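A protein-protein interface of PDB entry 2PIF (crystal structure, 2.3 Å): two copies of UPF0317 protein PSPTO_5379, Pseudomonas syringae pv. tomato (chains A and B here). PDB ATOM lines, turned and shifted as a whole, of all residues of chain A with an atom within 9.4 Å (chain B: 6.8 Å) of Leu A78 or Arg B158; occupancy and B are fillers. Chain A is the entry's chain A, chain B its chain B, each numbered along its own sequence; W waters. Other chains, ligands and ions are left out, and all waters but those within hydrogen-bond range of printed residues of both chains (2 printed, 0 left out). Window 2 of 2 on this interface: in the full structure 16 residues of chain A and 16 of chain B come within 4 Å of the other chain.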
ATOM      1  N   ARG A  19      -7.798 -33.804  11.579  1.00  0.00           N
ATOM      2  CA  ARG A  19      -6.889 -33.350  10.542  1.00  0.00           C
ATOM      3  C   ARG A  19      -5.552 -34.087  10.596  1.00  0.00           C
ATOM      4  O   ARG A  19      -4.765 -34.036   9.652  1.00  0.00           O
ATOM      5  CB  ARG A  19      -6.701 -31.827  10.597  1.00  0.00           C
ATOM      6  CG  ARG A  19      -6.324 -31.221  11.932  1.00  0.00           C
ATOM      7  CD  ARG A  19      -6.208 -29.694  11.765  1.00  0.00           C
ATOM      8  NE  ARG A  19      -5.517 -29.049  12.875  1.00  0.00           N
ATOM      9  CZ  ARG A  19      -6.082 -28.762  14.040  1.00  0.00           C
ATOM     10  NH1 ARG A  19      -7.364 -29.057  14.241  1.00  0.00           N
ATOM     11  NH2 ARG A  19      -5.366 -28.201  15.011  1.00  0.00           N
ATOM     12  N   ILE A  66     -13.867 -13.816   5.682  1.00  0.00           N
ATOM     13  CA  ILE A  66     -12.541 -14.322   5.992  1.00  0.00           C
ATOM     14  C   ILE A  66     -12.336 -14.672   7.475  1.00  0.00           C
ATOM     15  O   ILE A  66     -12.625 -13.859   8.363  1.00  0.00           O
ATOM     16  CB  ILE A  66     -11.469 -13.287   5.597  1.00  0.00           C
ATOM     17  CG1 ILE A  66     -11.454 -13.087   4.080  1.00  0.00           C
ATOM     18  CG2 ILE A  66     -10.104 -13.745   6.069  1.00  0.00           C
ATOM     19  CD1 ILE A  66     -10.319 -12.192   3.603  1.00  0.00           C
ATOM     20  N   LEU A  67     -11.857 -15.887   7.740  1.00  0.00           N
ATOM     21  CA  LEU A  67     -11.550 -16.297   9.112  1.00  0.00           C
ATOM     22  C   LEU A  67     -10.069 -15.985   9.306  1.00  0.00           C
ATOM     23  O   LEU A  67      -9.635 -15.577  10.386  1.00  0.00           O
ATOM     24  CB  LEU A  67     -11.800 -17.792   9.317  1.00  0.00           C
ATOM     25  CG  LEU A  67     -13.262 -18.248   9.281  1.00  0.00           C
ATOM     26  CD1 LEU A  67     -13.309 -19.774   9.280  1.00  0.00           C
ATOM     27  CD2 LEU A  67     -14.040 -17.659  10.482  1.00  0.00           C
ATOM     28  N   ASP A  68      -9.287 -16.171   8.244  1.00  0.00           N
ATOM     29  CA  ASP A  68      -7.865 -15.864   8.322  1.00  0.00           C
ATOM     30  C   ASP A  68      -7.180 -15.875   6.971  1.00  0.00           C
ATOM     31  O   ASP A  68      -7.649 -16.488   6.016  1.00  0.00           O
ATOM     32  CB  ASP A  68      -7.158 -16.841   9.259  1.00  0.00           C
ATOM     33  CG  ASP A  68      -5.950 -16.220   9.940  1.00  0.00           C
ATOM     34  OD1 ASP A  68      -6.096 -15.122  10.531  1.00  0.00           O
ATOM     35  OD2 ASP A  68      -4.857 -16.834   9.889  1.00  0.00           O
ATOM     36  N   VAL A  69      -6.062 -15.169   6.901  1.00  0.00           N
ATOM     37  CA  VAL A  69      -5.278 -15.085   5.685  1.00  0.00           C
ATOM     38  C   VAL A  69      -3.853 -15.368   6.107  1.00  0.00           C
ATOM     39  O   VAL A  69      -3.301 -14.653   6.943  1.00  0.00           O
ATOM     40  CB  VAL A  69      -5.294 -13.675   5.101  1.00  0.00           C
ATOM     41  CG1 VAL A  69      -4.594 -13.678   3.731  1.00  0.00           C
ATOM     42  CG2 VAL A  69      -6.735 -13.155   5.033  1.00  0.00           C
ATOM     43  N   SER A  70      -3.254 -16.402   5.524  1.00  0.00           N
ATOM     44  CA  SER A  70      -1.880 -16.774   5.852  1.00  0.00           C
ATOM     45  C   SER A  70      -0.913 -15.775   5.235  1.00  0.00           C
ATOM     46  O   SER A  70      -1.288 -15.004   4.359  1.00  0.00           O
ATOM     47  CB  SER A  70      -1.574 -18.178   5.310  1.00  0.00           C
ATOM     48  OG  SER A  70      -1.468 -18.163   3.889  1.00  0.00           O
ATOM     49  N   ASP A  71       0.331 -15.784   5.700  1.00  0.00           N
ATOM     50  CA  ASP A  71       1.333 -14.894   5.129  1.00  0.00           C
ATOM     51  C   ASP A  71       1.705 -15.510   3.781  1.00  0.00           C
ATOM     52  O   ASP A  71       1.357 -16.664   3.510  1.00  0.00           O
ATOM     53  CB  ASP A  71       2.577 -14.802   6.025  1.00  0.00           C
ATOM     54  CG  ASP A  71       2.270 -14.222   7.401  1.00  0.00           C
ATOM     55  OD1 ASP A  71       1.362 -13.368   7.502  1.00  0.00           O
ATOM     56  OD2 ASP A  71       2.951 -14.602   8.375  1.00  0.00           O
ATOM     57  N   PRO A  75       2.000 -22.748   4.669  1.00  0.00           N
ATOM     58  CA  PRO A  75       0.635 -22.799   5.196  1.00  0.00           C
ATOM     59  C   PRO A  75       0.557 -22.184   6.580  1.00  0.00           C
ATOM     60  O   PRO A  75       0.864 -21.008   6.755  1.00  0.00           O
ATOM     61  CB  PRO A  75       0.329 -24.291   5.213  1.00  0.00           C
ATOM     62  CG  PRO A  75       1.645 -24.877   5.552  1.00  0.00           C
ATOM     63  CD  PRO A  75       2.587 -24.100   4.651  1.00  0.00           C
ATOM     64  N   THR A  76       0.161 -22.990   7.558  1.00  0.00           N
ATOM     65  CA  THR A  76       0.022 -22.540   8.942  1.00  0.00           C
ATOM     66  C   THR A  76      -0.988 -21.407   9.071  1.00  0.00           C
ATOM     67  O   THR A  76      -0.975 -20.438   8.306  1.00  0.00           O
ATOM     68  CB  THR A  76       1.378 -22.063   9.558  1.00  0.00           C
ATOM     69  OG1 THR A  76       1.785 -20.823   8.962  1.00  0.00           O
ATOM     70  CG2 THR A  76       2.468 -23.111   9.343  1.00  0.00           C
ATOM     71  N   THR A  77      -1.872 -21.548  10.048  1.00  0.00           N
ATOM     72  CA  THR A  77      -2.896 -20.558  10.324  1.00  0.00           C
ATOM     73  C   THR A  77      -3.147 -20.515  11.819  1.00  0.00           C
ATOM     74  O   THR A  77      -3.065 -21.538  12.508  1.00  0.00           O
ATOM     75  CB  THR A  77      -4.223 -20.878   9.605  1.00  0.00           C
ATOM     76  OG1 THR A  77      -5.270 -20.087  10.180  1.00  0.00           O
ATOM     77  CG2 THR A  77      -4.574 -22.348   9.743  1.00  0.00           C
ATOM     78  N   LEU A  78      -3.453 -19.325  12.318  1.00  0.00           N
ATOM     79  CA  LEU A  78      -3.707 -19.136  13.734  1.00  0.00           C
ATOM     80  C   LEU A  78      -4.951 -19.873  14.214  1.00  0.00           C
ATOM     81  O   LEU A  78      -5.180 -19.985  15.418  1.00  0.00           O
ATOM     82  CB  LEU A  78      -3.835 -17.649  14.029  1.00  0.00           C
ATOM     83  CG  LEU A  78      -2.612 -16.852  13.590  1.00  0.00           C
ATOM     84  CD1 LEU A  78      -2.870 -15.365  13.803  1.00  0.00           C
ATOM     85  CD2 LEU A  78      -1.380 -17.324  14.363  1.00  0.00           C
ATOM     86  N   LEU A  79      -5.747 -20.380  13.278  1.00  0.00           N
ATOM     87  CA  LEU A  79      -6.970 -21.103  13.623  1.00  0.00           C
ATOM     88  C   LEU A  79      -6.663 -22.524  14.089  1.00  0.00           C
ATOM     89  O   LEU A  79      -7.519 -23.192  14.677  1.00  0.00           O
ATOM     90  CB  LEU A  79      -7.907 -21.158  12.415  1.00  0.00           C
ATOM     91  CG  LEU A  79      -8.648 -19.886  11.986  1.00  0.00           C
ATOM     92  CD1 LEU A  79      -7.763 -18.648  12.130  1.00  0.00           C
ATOM     93  CD2 LEU A  79      -9.109 -20.066  10.536  1.00  0.00           C
ATOM     94  N   ALA A  80      -5.446 -22.984  13.812  1.00  0.00           N
ATOM     95  CA  ALA A  80      -5.024 -24.330  14.204  1.00  0.00           C
ATOM     96  C   ALA A  80      -3.506 -24.380  14.339  1.00  0.00           C
ATOM     97  O   ALA A  80      -2.792 -24.632  13.370  1.00  0.00           O
ATOM     98  CB  ALA A  80      -5.493 -25.341  13.172  1.00  0.00           C
ATOM     99  N   GLU A  81      -3.018 -24.125  15.547  1.00  0.00           N
ATOM    100  CA  GLU A  81      -1.585 -24.126  15.814  1.00  0.00           C
ATOM    101  C   GLU A  81      -0.964 -25.463  15.399  1.00  0.00           C
ATOM    102  O   GLU A  81      -1.500 -26.529  15.713  1.00  0.00           O
ATOM    103  CB  GLU A  81      -1.346 -23.866  17.305  1.00  0.00           C
ATOM    104  CG  GLU A  81       0.077 -23.454  17.681  1.00  0.00           C
ATOM    105  CD  GLU A  81       0.449 -22.050  17.200  1.00  0.00           C
ATOM    106  OE1 GLU A  81      -0.367 -21.117  17.374  1.00  0.00           O
ATOM    107  OE2 GLU A  81       1.566 -21.879  16.657  1.00  0.00           O
ATOM    108  N   GLY A  82       0.153 -25.390  14.674  1.00  0.00           N
ATOM    109  CA  GLY A  82       0.851 -26.587  14.233  1.00  0.00           C
ATOM    110  C   GLY A  82       0.263 -27.311  13.035  1.00  0.00           C
ATOM    111  O   GLY A  82       0.772 -28.353  12.616  1.00  0.00           O
ATOM    112  N   SER A  83      -0.807 -26.766  12.474  1.00  0.00           N
ATOM    113  CA  SER A  83      -1.449 -27.388  11.325  1.00  0.00           C
ATOM    114  C   SER A  83      -0.752 -27.002  10.026  1.00  0.00           C
ATOM    115  O   SER A  83      -0.080 -25.979   9.956  1.00  0.00           O
ATOM    116  CB  SER A  83      -2.915 -26.968  11.266  1.00  0.00           C
ATOM    117  OG  SER A  83      -3.042 -25.564  11.127  1.00  0.00           O
ATOM    118  N   LEU A  85      -1.757 -26.444   6.120  1.00  0.00           N
ATOM    119  CA  LEU A  85      -2.855 -26.308   5.170  1.00  0.00           C
ATOM    120  C   LEU A  85      -2.722 -27.177   3.913  1.00  0.00           C
ATOM    121  O   LEU A  85      -3.707 -27.446   3.219  1.00  0.00           O
ATOM    122  CB  LEU A  85      -3.011 -24.824   4.799  1.00  0.00           C
ATOM    123  CG  LEU A  85      -3.361 -23.907   5.985  1.00  0.00           C
ATOM    124  CD1 LEU A  85      -3.091 -22.454   5.649  1.00  0.00           C
ATOM    125  CD2 LEU A  85      -4.820 -24.116   6.369  1.00  0.00           C
ATOM    126  N   ALA A 119      -2.931 -18.311   1.453  1.00  0.00           N
ATOM    127  CA  ALA A 119      -4.072 -19.115   1.880  1.00  0.00           C
ATOM    128  C   ALA A 119      -5.159 -18.298   2.588  1.00  0.00           C
ATOM    129  O   ALA A 119      -4.886 -17.565   3.535  1.00  0.00           O
ATOM    130  CB  ALA A 119      -3.594 -20.230   2.801  1.00  0.00           C
ATOM    131  N   LEU A 121      -8.683 -18.712   4.653  1.00  0.00           N
ATOM    132  CA  LEU A 121      -9.605 -19.634   5.319  1.00  0.00           C
ATOM    133  C   LEU A 121     -10.919 -18.890   5.457  1.00  0.00           C
ATOM    134  O   LEU A 121     -11.016 -17.890   6.177  1.00  0.00           O
ATOM    135  CB  LEU A 121      -9.070 -20.066   6.691  1.00  0.00           C
ATOM    136  CG  LEU A 121      -7.865 -21.011   6.610  1.00  0.00           C
ATOM    137  CD1 LEU A 121      -7.580 -21.625   7.969  1.00  0.00           C
ATOM    138  CD2 LEU A 121      -8.159 -22.112   5.619  1.00  0.00           C
ATOM    139  N   PHE A 257     -11.650 -27.718   6.140  1.00  0.00           N
ATOM    140  CA  PHE A 257     -10.558 -27.623   7.091  1.00  0.00           C
ATOM    141  C   PHE A 257     -11.168 -27.392   8.470  1.00  0.00           C
ATOM    142  O   PHE A 257     -11.796 -26.360   8.713  1.00  0.00           O
ATOM    143  CB  PHE A 257      -9.648 -26.446   6.725  1.00  0.00           C
ATOM    144  CG  PHE A 257      -8.561 -26.180   7.729  1.00  0.00           C
ATOM    145  CD1 PHE A 257      -7.418 -26.970   7.765  1.00  0.00           C
ATOM    146  CD2 PHE A 257      -8.682 -25.139   8.649  1.00  0.00           C
ATOM    147  CE1 PHE A 257      -6.414 -26.729   8.697  1.00  0.00           C
ATOM    148  CE2 PHE A 257      -7.674 -24.895   9.586  1.00  0.00           C
ATOM    149  CZ  PHE A 257      -6.537 -25.696   9.608  1.00  0.00           C
ATOM    150  N   THR A 259     -10.889 -26.305  12.041  1.00  0.00           N
ATOM    151  CA  THR A 259      -9.982 -25.472  12.831  1.00  0.00           C
ATOM    152  C   THR A 259     -10.048 -25.799  14.319  1.00  0.00           C
ATOM    153  O   THR A 259     -10.709 -26.751  14.723  1.00  0.00           O
ATOM    154  CB  THR A 259     -10.313 -23.973  12.668  1.00  0.00           C
ATOM    155  OG1 THR A 259     -11.477 -23.651  13.443  1.00  0.00           O
ATOM    156  CG2 THR A 259     -10.572 -23.646  11.210  1.00  0.00           C
ATOM    157  N   ASP A 260      -9.360 -24.999  15.127  1.00  0.00           N
ATOM    158  CA  ASP A 260      -9.362 -25.189  16.571  1.00  0.00           C
ATOM    159  C   ASP A 260     -10.314 -24.197  17.249  1.00  0.00           C
ATOM    160  O   ASP A 260     -10.349 -24.107  18.481  1.00  0.00           O
ATOM    161  CB  ASP A 260      -7.954 -25.007  17.168  1.00  0.00           C
ATOM    162  CG  ASP A 260      -7.001 -26.151  16.822  1.00  0.00           C
ATOM    163  OD1 ASP A 260      -7.455 -27.314  16.674  1.00  0.00           O
ATOM    164  OD2 ASP A 260      -5.787 -25.885  16.720  1.00  0.00           O
ATOM    165  N   VAL A 261     -11.079 -23.457  16.449  1.00  0.00           N
ATOM    166  CA  VAL A 261     -12.015 -22.460  16.982  1.00  0.00           C
ATOM    167  C   VAL A 261     -13.417 -23.032  17.143  1.00  0.00           C
ATOM    168  O   VAL A 261     -14.024 -23.493  16.180  1.00  0.00           O
ATOM    169  CB  VAL A 261     -12.076 -21.218  16.064  1.00  0.00           C
ATOM    170  CG1 VAL A 261     -12.979 -20.144  16.674  1.00  0.00           C
ATOM    171  CG2 VAL A 261     -10.662 -20.679  15.840  1.00  0.00           C
ATOM    172  N   LEU B  55      -4.297  -5.990   3.664  1.00  0.00           N
ATOM    173  CA  LEU B  55      -4.129  -7.092   4.618  1.00  0.00           C
ATOM    174  C   LEU B  55      -3.885  -6.524   6.017  1.00  0.00           C
ATOM    175  O   LEU B  55      -4.247  -7.140   7.024  1.00  0.00           O
ATOM    176  CB  LEU B  55      -2.944  -7.985   4.228  1.00  0.00           C
ATOM    177  CG  LEU B  55      -2.585  -9.135   5.183  1.00  0.00           C
ATOM    178  CD1 LEU B  55      -3.744 -10.111   5.263  1.00  0.00           C
ATOM    179  CD2 LEU B  55      -1.331  -9.871   4.701  1.00  0.00           C
ATOM    180  N   TYR B  56      -3.264  -5.349   6.070  1.00  0.00           N
ATOM    181  CA  TYR B  56      -2.989  -4.693   7.340  1.00  0.00           C
ATOM    182  C   TYR B  56      -4.343  -4.311   7.924  1.00  0.00           C
ATOM    183  O   TYR B  56      -4.575  -4.419   9.123  1.00  0.00           O
ATOM    184  CB  TYR B  56      -2.133  -3.446   7.106  1.00  0.00           C
ATOM    185  CG  TYR B  56      -1.511  -2.810   8.342  1.00  0.00           C
ATOM    186  CD1 TYR B  56      -0.674  -3.534   9.191  1.00  0.00           C
ATOM    187  CD2 TYR B  56      -1.701  -1.455   8.612  1.00  0.00           C
ATOM    188  CE1 TYR B  56      -0.035  -2.922  10.276  1.00  0.00           C
ATOM    189  CE2 TYR B  56      -1.070  -0.827   9.693  1.00  0.00           C
ATOM    190  CZ  TYR B  56      -0.241  -1.566  10.517  1.00  0.00           C
ATOM    191  OH  TYR B  56       0.369  -0.941  11.574  1.00  0.00           O
ATOM    192  N   GLN B  58      -7.389  -5.775   7.169  1.00  0.00           N
ATOM    193  CA  GLN B  58      -8.173  -6.937   7.551  1.00  0.00           C
ATOM    194  C   GLN B  58      -7.678  -7.503   8.878  1.00  0.00           C
ATOM    195  O   GLN B  58      -8.449  -8.109   9.623  1.00  0.00           O
ATOM    196  CB  GLN B  58      -8.164  -7.998   6.436  1.00  0.00           C
ATOM    197  CG  GLN B  58      -7.228  -9.206   6.607  1.00  0.00           C
ATOM    198  CD  GLN B  58      -7.704 -10.223   7.640  1.00  0.00           C
ATOM    199  OE1 GLN B  58      -8.892 -10.318   7.947  1.00  0.00           O
ATOM    200  NE2 GLN B  58      -6.772 -10.996   8.166  1.00  0.00           N
ATOM    201  N   ARG B  59      -6.409  -7.262   9.195  1.00  0.00           N
ATOM    202  CA  ARG B  59      -5.831  -7.749  10.440  1.00  0.00           C
ATOM    203  C   ARG B  59      -5.978  -6.804  11.632  1.00  0.00           C
ATOM    204  O   ARG B  59      -5.858  -7.239  12.787  1.00  0.00           O
ATOM    205  CB  ARG B  59      -4.346  -8.085  10.237  1.00  0.00           C
ATOM    206  CG  ARG B  59      -4.133  -9.353   9.446  1.00  0.00           C
ATOM    207  CD  ARG B  59      -2.669  -9.690   9.214  1.00  0.00           C
ATOM    208  NE  ARG B  59      -2.573 -10.969   8.515  1.00  0.00           N
ATOM    209  CZ  ARG B  59      -1.435 -11.526   8.116  1.00  0.00           C
ATOM    210  NH1 ARG B  59      -0.281 -10.912   8.340  1.00  0.00           N
ATOM    211  NH2 ARG B  59      -1.450 -12.710   7.498  1.00  0.00           N
ATOM    212  N   ASN B  60      -6.235  -5.526  11.352  1.00  0.00           N
ATOM    213  CA  ASN B  60      -6.384  -4.495  12.389  1.00  0.00           C
ATOM    214  C   ASN B  60      -7.625  -3.633  12.116  1.00  0.00           C
ATOM    215  O   ASN B  60      -7.523  -2.421  11.889  1.00  0.00           O
ATOM    216  CB  ASN B  60      -5.147  -3.597  12.400  1.00  0.00           C
ATOM    217  CG  ASN B  60      -3.863  -4.376  12.584  1.00  0.00           C
ATOM    218  OD1 ASN B  60      -3.614  -4.946  13.646  1.00  0.00           O
ATOM    219  ND2 ASN B  60      -3.044  -4.411  11.547  1.00  0.00           N
ATOM    220  N   ALA B 156       1.546  -2.128  19.237  1.00  0.00           N
ATOM    221  CA  ALA B 156       1.800  -2.484  17.852  1.00  0.00           C
ATOM    222  C   ALA B 156       0.630  -3.176  17.179  1.00  0.00           C
ATOM    223  O   ALA B 156      -0.079  -3.978  17.793  1.00  0.00           O
ATOM    224  CB  ALA B 156       3.047  -3.371  17.764  1.00  0.00           C
ATOM    225  N   CYS B 157       0.434  -2.844  15.906  1.00  0.00           N
ATOM    226  CA  CYS B 157      -0.617  -3.451  15.098  1.00  0.00           C
ATOM    227  C   CYS B 157      -0.087  -4.818  14.664  1.00  0.00           C
ATOM    228  O   CYS B 157       1.135  -5.029  14.605  1.00  0.00           O
ATOM    229  CB  CYS B 157      -0.885  -2.614  13.840  1.00  0.00           C
ATOM    230  SG  CYS B 157      -1.614  -0.967  14.086  1.00  0.00           S
ATOM    231  N   ARG B 158      -0.988  -5.748  14.370  1.00  0.00           N
ATOM    232  CA  ARG B 158      -0.550  -7.050  13.902  1.00  0.00           C
ATOM    233  C   ARG B 158       0.105  -6.767  12.555  1.00  0.00           C
ATOM    234  O   ARG B 158      -0.431  -6.005  11.750  1.00  0.00           O
ATOM    235  CB  ARG B 158      -1.739  -7.996  13.722  1.00  0.00           C
ATOM    236  CG  ARG B 158      -1.359  -9.287  13.023  1.00  0.00           C
ATOM    237  CD  ARG B 158      -2.500 -10.289  12.942  1.00  0.00           C
ATOM    238  NE  ARG B 158      -2.104 -11.433  12.119  1.00  0.00           N
ATOM    239  CZ  ARG B 158      -2.894 -12.458  11.814  1.00  0.00           C
ATOM    240  NH1 ARG B 158      -4.141 -12.504  12.267  1.00  0.00           N
ATOM    241  NH2 ARG B 158      -2.439 -13.429  11.033  1.00  0.00           N
ATOM    242  N   PRO B 159       1.296  -7.339  12.311  1.00  0.00           N
ATOM    243  CA  PRO B 159       2.007  -7.131  11.043  1.00  0.00           C
ATOM    244  C   PRO B 159       1.284  -7.738   9.848  1.00  0.00           C
ATOM    245  O   PRO B 159       0.535  -8.708   9.985  1.00  0.00           O
ATOM    246  CB  PRO B 159       3.363  -7.784  11.292  1.00  0.00           C
ATOM    247  CG  PRO B 159       3.035  -8.866  12.289  1.00  0.00           C
ATOM    248  CD  PRO B 159       2.106  -8.152  13.236  1.00  0.00           C
ATOM    249  N   ALA B 160       1.514  -7.152   8.681  1.00  0.00           N
ATOM    250  CA  ALA B 160       0.898  -7.606   7.436  1.00  0.00           C
ATOM    251  C   ALA B 160       1.887  -7.382   6.295  1.00  0.00           C
ATOM    252  O   ALA B 160       2.146  -6.249   5.898  1.00  0.00           O
ATOM    253  CB  ALA B 160      -0.395  -6.829   7.176  1.00  0.00           C
ATOM    254  N   LEU B 163       4.339  -4.290   6.063  1.00  0.00           N
ATOM    255  CA  LEU B 163       3.878  -3.264   6.979  1.00  0.00           C
ATOM    256  C   LEU B 163       3.859  -3.663   8.446  1.00  0.00           C
ATOM    257  O   LEU B 163       3.529  -4.800   8.805  1.00  0.00           O
ATOM    258  CB  LEU B 163       2.475  -2.818   6.567  1.00  0.00           C
ATOM    259  CG  LEU B 163       2.283  -2.208   5.187  1.00  0.00           C
ATOM    260  CD1 LEU B 163       0.806  -1.892   5.002  1.00  0.00           C
ATOM    261  CD2 LEU B 163       3.121  -0.940   5.041  1.00  0.00           C
ATOM    262  N   HIS B 164       4.210  -2.711   9.296  1.00  0.00           N
ATOM    263  CA  HIS B 164       4.194  -2.925  10.731  1.00  0.00           C
ATOM    264  C   HIS B 164       4.140  -1.537  11.354  1.00  0.00           C
ATOM    265  O   HIS B 164       4.539  -0.559  10.722  1.00  0.00           O
ATOM    266  CB  HIS B 164       5.434  -3.710  11.176  1.00  0.00           C
ATOM    267  CG  HIS B 164       6.737  -3.060  10.818  1.00  0.00           C
ATOM    268  ND1 HIS B 164       7.367  -2.150  11.641  1.00  0.00           N
ATOM    269  CD2 HIS B 164       7.530  -3.192   9.726  1.00  0.00           C
ATOM    270  CE1 HIS B 164       8.493  -1.754  11.074  1.00  0.00           C
ATOM    271  NE2 HIS B 164       8.615  -2.371   9.911  1.00  0.00           N
ATOM    272  N   GLY B 165       3.624  -1.427  12.570  1.00  0.00           N
ATOM    273  CA  GLY B 165       3.550  -0.114  13.176  1.00  0.00           C
ATOM    274  C   GLY B 165       2.601  -0.040  14.351  1.00  0.00           C
ATOM    275  O   GLY B 165       1.822  -0.954  14.595  1.00  0.00           O
HETATM  276  O   HOH W   1      -2.569 -15.344   9.296  1.00  0.00           O
HETATM  277  O   HOH W   2      -4.823 -12.484   8.504  1.00  0.00           O
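OD1 of Asp A68 lies within salt-bridge range of NH1 of Arg B158 (3.7 Å).
The backbone carbonyl oxygen (O) of Val A69 lies within hydrogen-bond range of the guanidinium group (NH2) of Arg B59, at 2.7 Å.
OD1 of Asp A71 lies within salt-bridge range of NH2 of Arg B59 (2.9 Å).
The side-chain hydroxyl (OG1) of Thr A77 is in hydrogen-bond range of the side-chain carboxylate (OD2) of Asp A68.
The backbone NH (N) of Leu A121 lies within hydrogen-bond range of the backbone carbonyl oxygen (O) of Asp A68, 2.8 Å away.
O of Ala A119 lies within hydrogen-bond range of N of Ser A70.
The backbone carbonyl oxygen of Pro B159 is in hydrogen-bond range of the guanidinium group of Arg B59 (2.9 Å).
N of Arg B158 lies within hydrogen-bond range of OD1 of Asn B60, 2.8 Å away.
Among the printed residues, merely in contact across the chains: Val A69 with Leu B55 (3.9 Å), Val A69 with Gln B58 (3.8 Å), Ser A70 with Arg B59 (3.8 Å) and Leu A78 with Arg B158 (3.4 Å).
Of the printed residues of chain B, Ser A70 touches Arg B59 (3.8 Å).
Of chain B, only Arg B158 comes within 4 Å of Leu A78.
Leu A85 touches none of the printed residues of chain B.
Of the printed residues of chain A, Leu B55 touches Val A69 (3.9 Å).
No residue of chain A comes within 4 Å of Pro B159.
Of the 23 printed residues of chain A, 5 touch a printed residue of chain B.
Printed residues of chain A that touch a printed residue of chain B: Asp A68, Val A69, Ser A70, Asp A71 and Leu A78.
Hydrophobic or aromatic side chains of chain A within 4 Å of the printed part of chain B: Val A69 and Leu A78.
Hydrophobic or aromatic side chains of chain B that line the printed part of chain A: Leu B55.
Among the printed residues, 7 pairs touch across the chains.
No position is printed for both chains.
Water W2 lies within hydrogen-bond range of the side-chain amide nitrogen (NE2) of Gln B58 (2.5 Å), the guanidinium group (NE) of Arg B59 (2.7 Å) and the backbone carbonyl oxygen (O) of Val A69 (3.1 Å).
Water W1 lies within hydrogen-bond range of O of Val A69, NH2 of Arg B158, OD2 of Asp A68 and NH2 of Arg B59.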
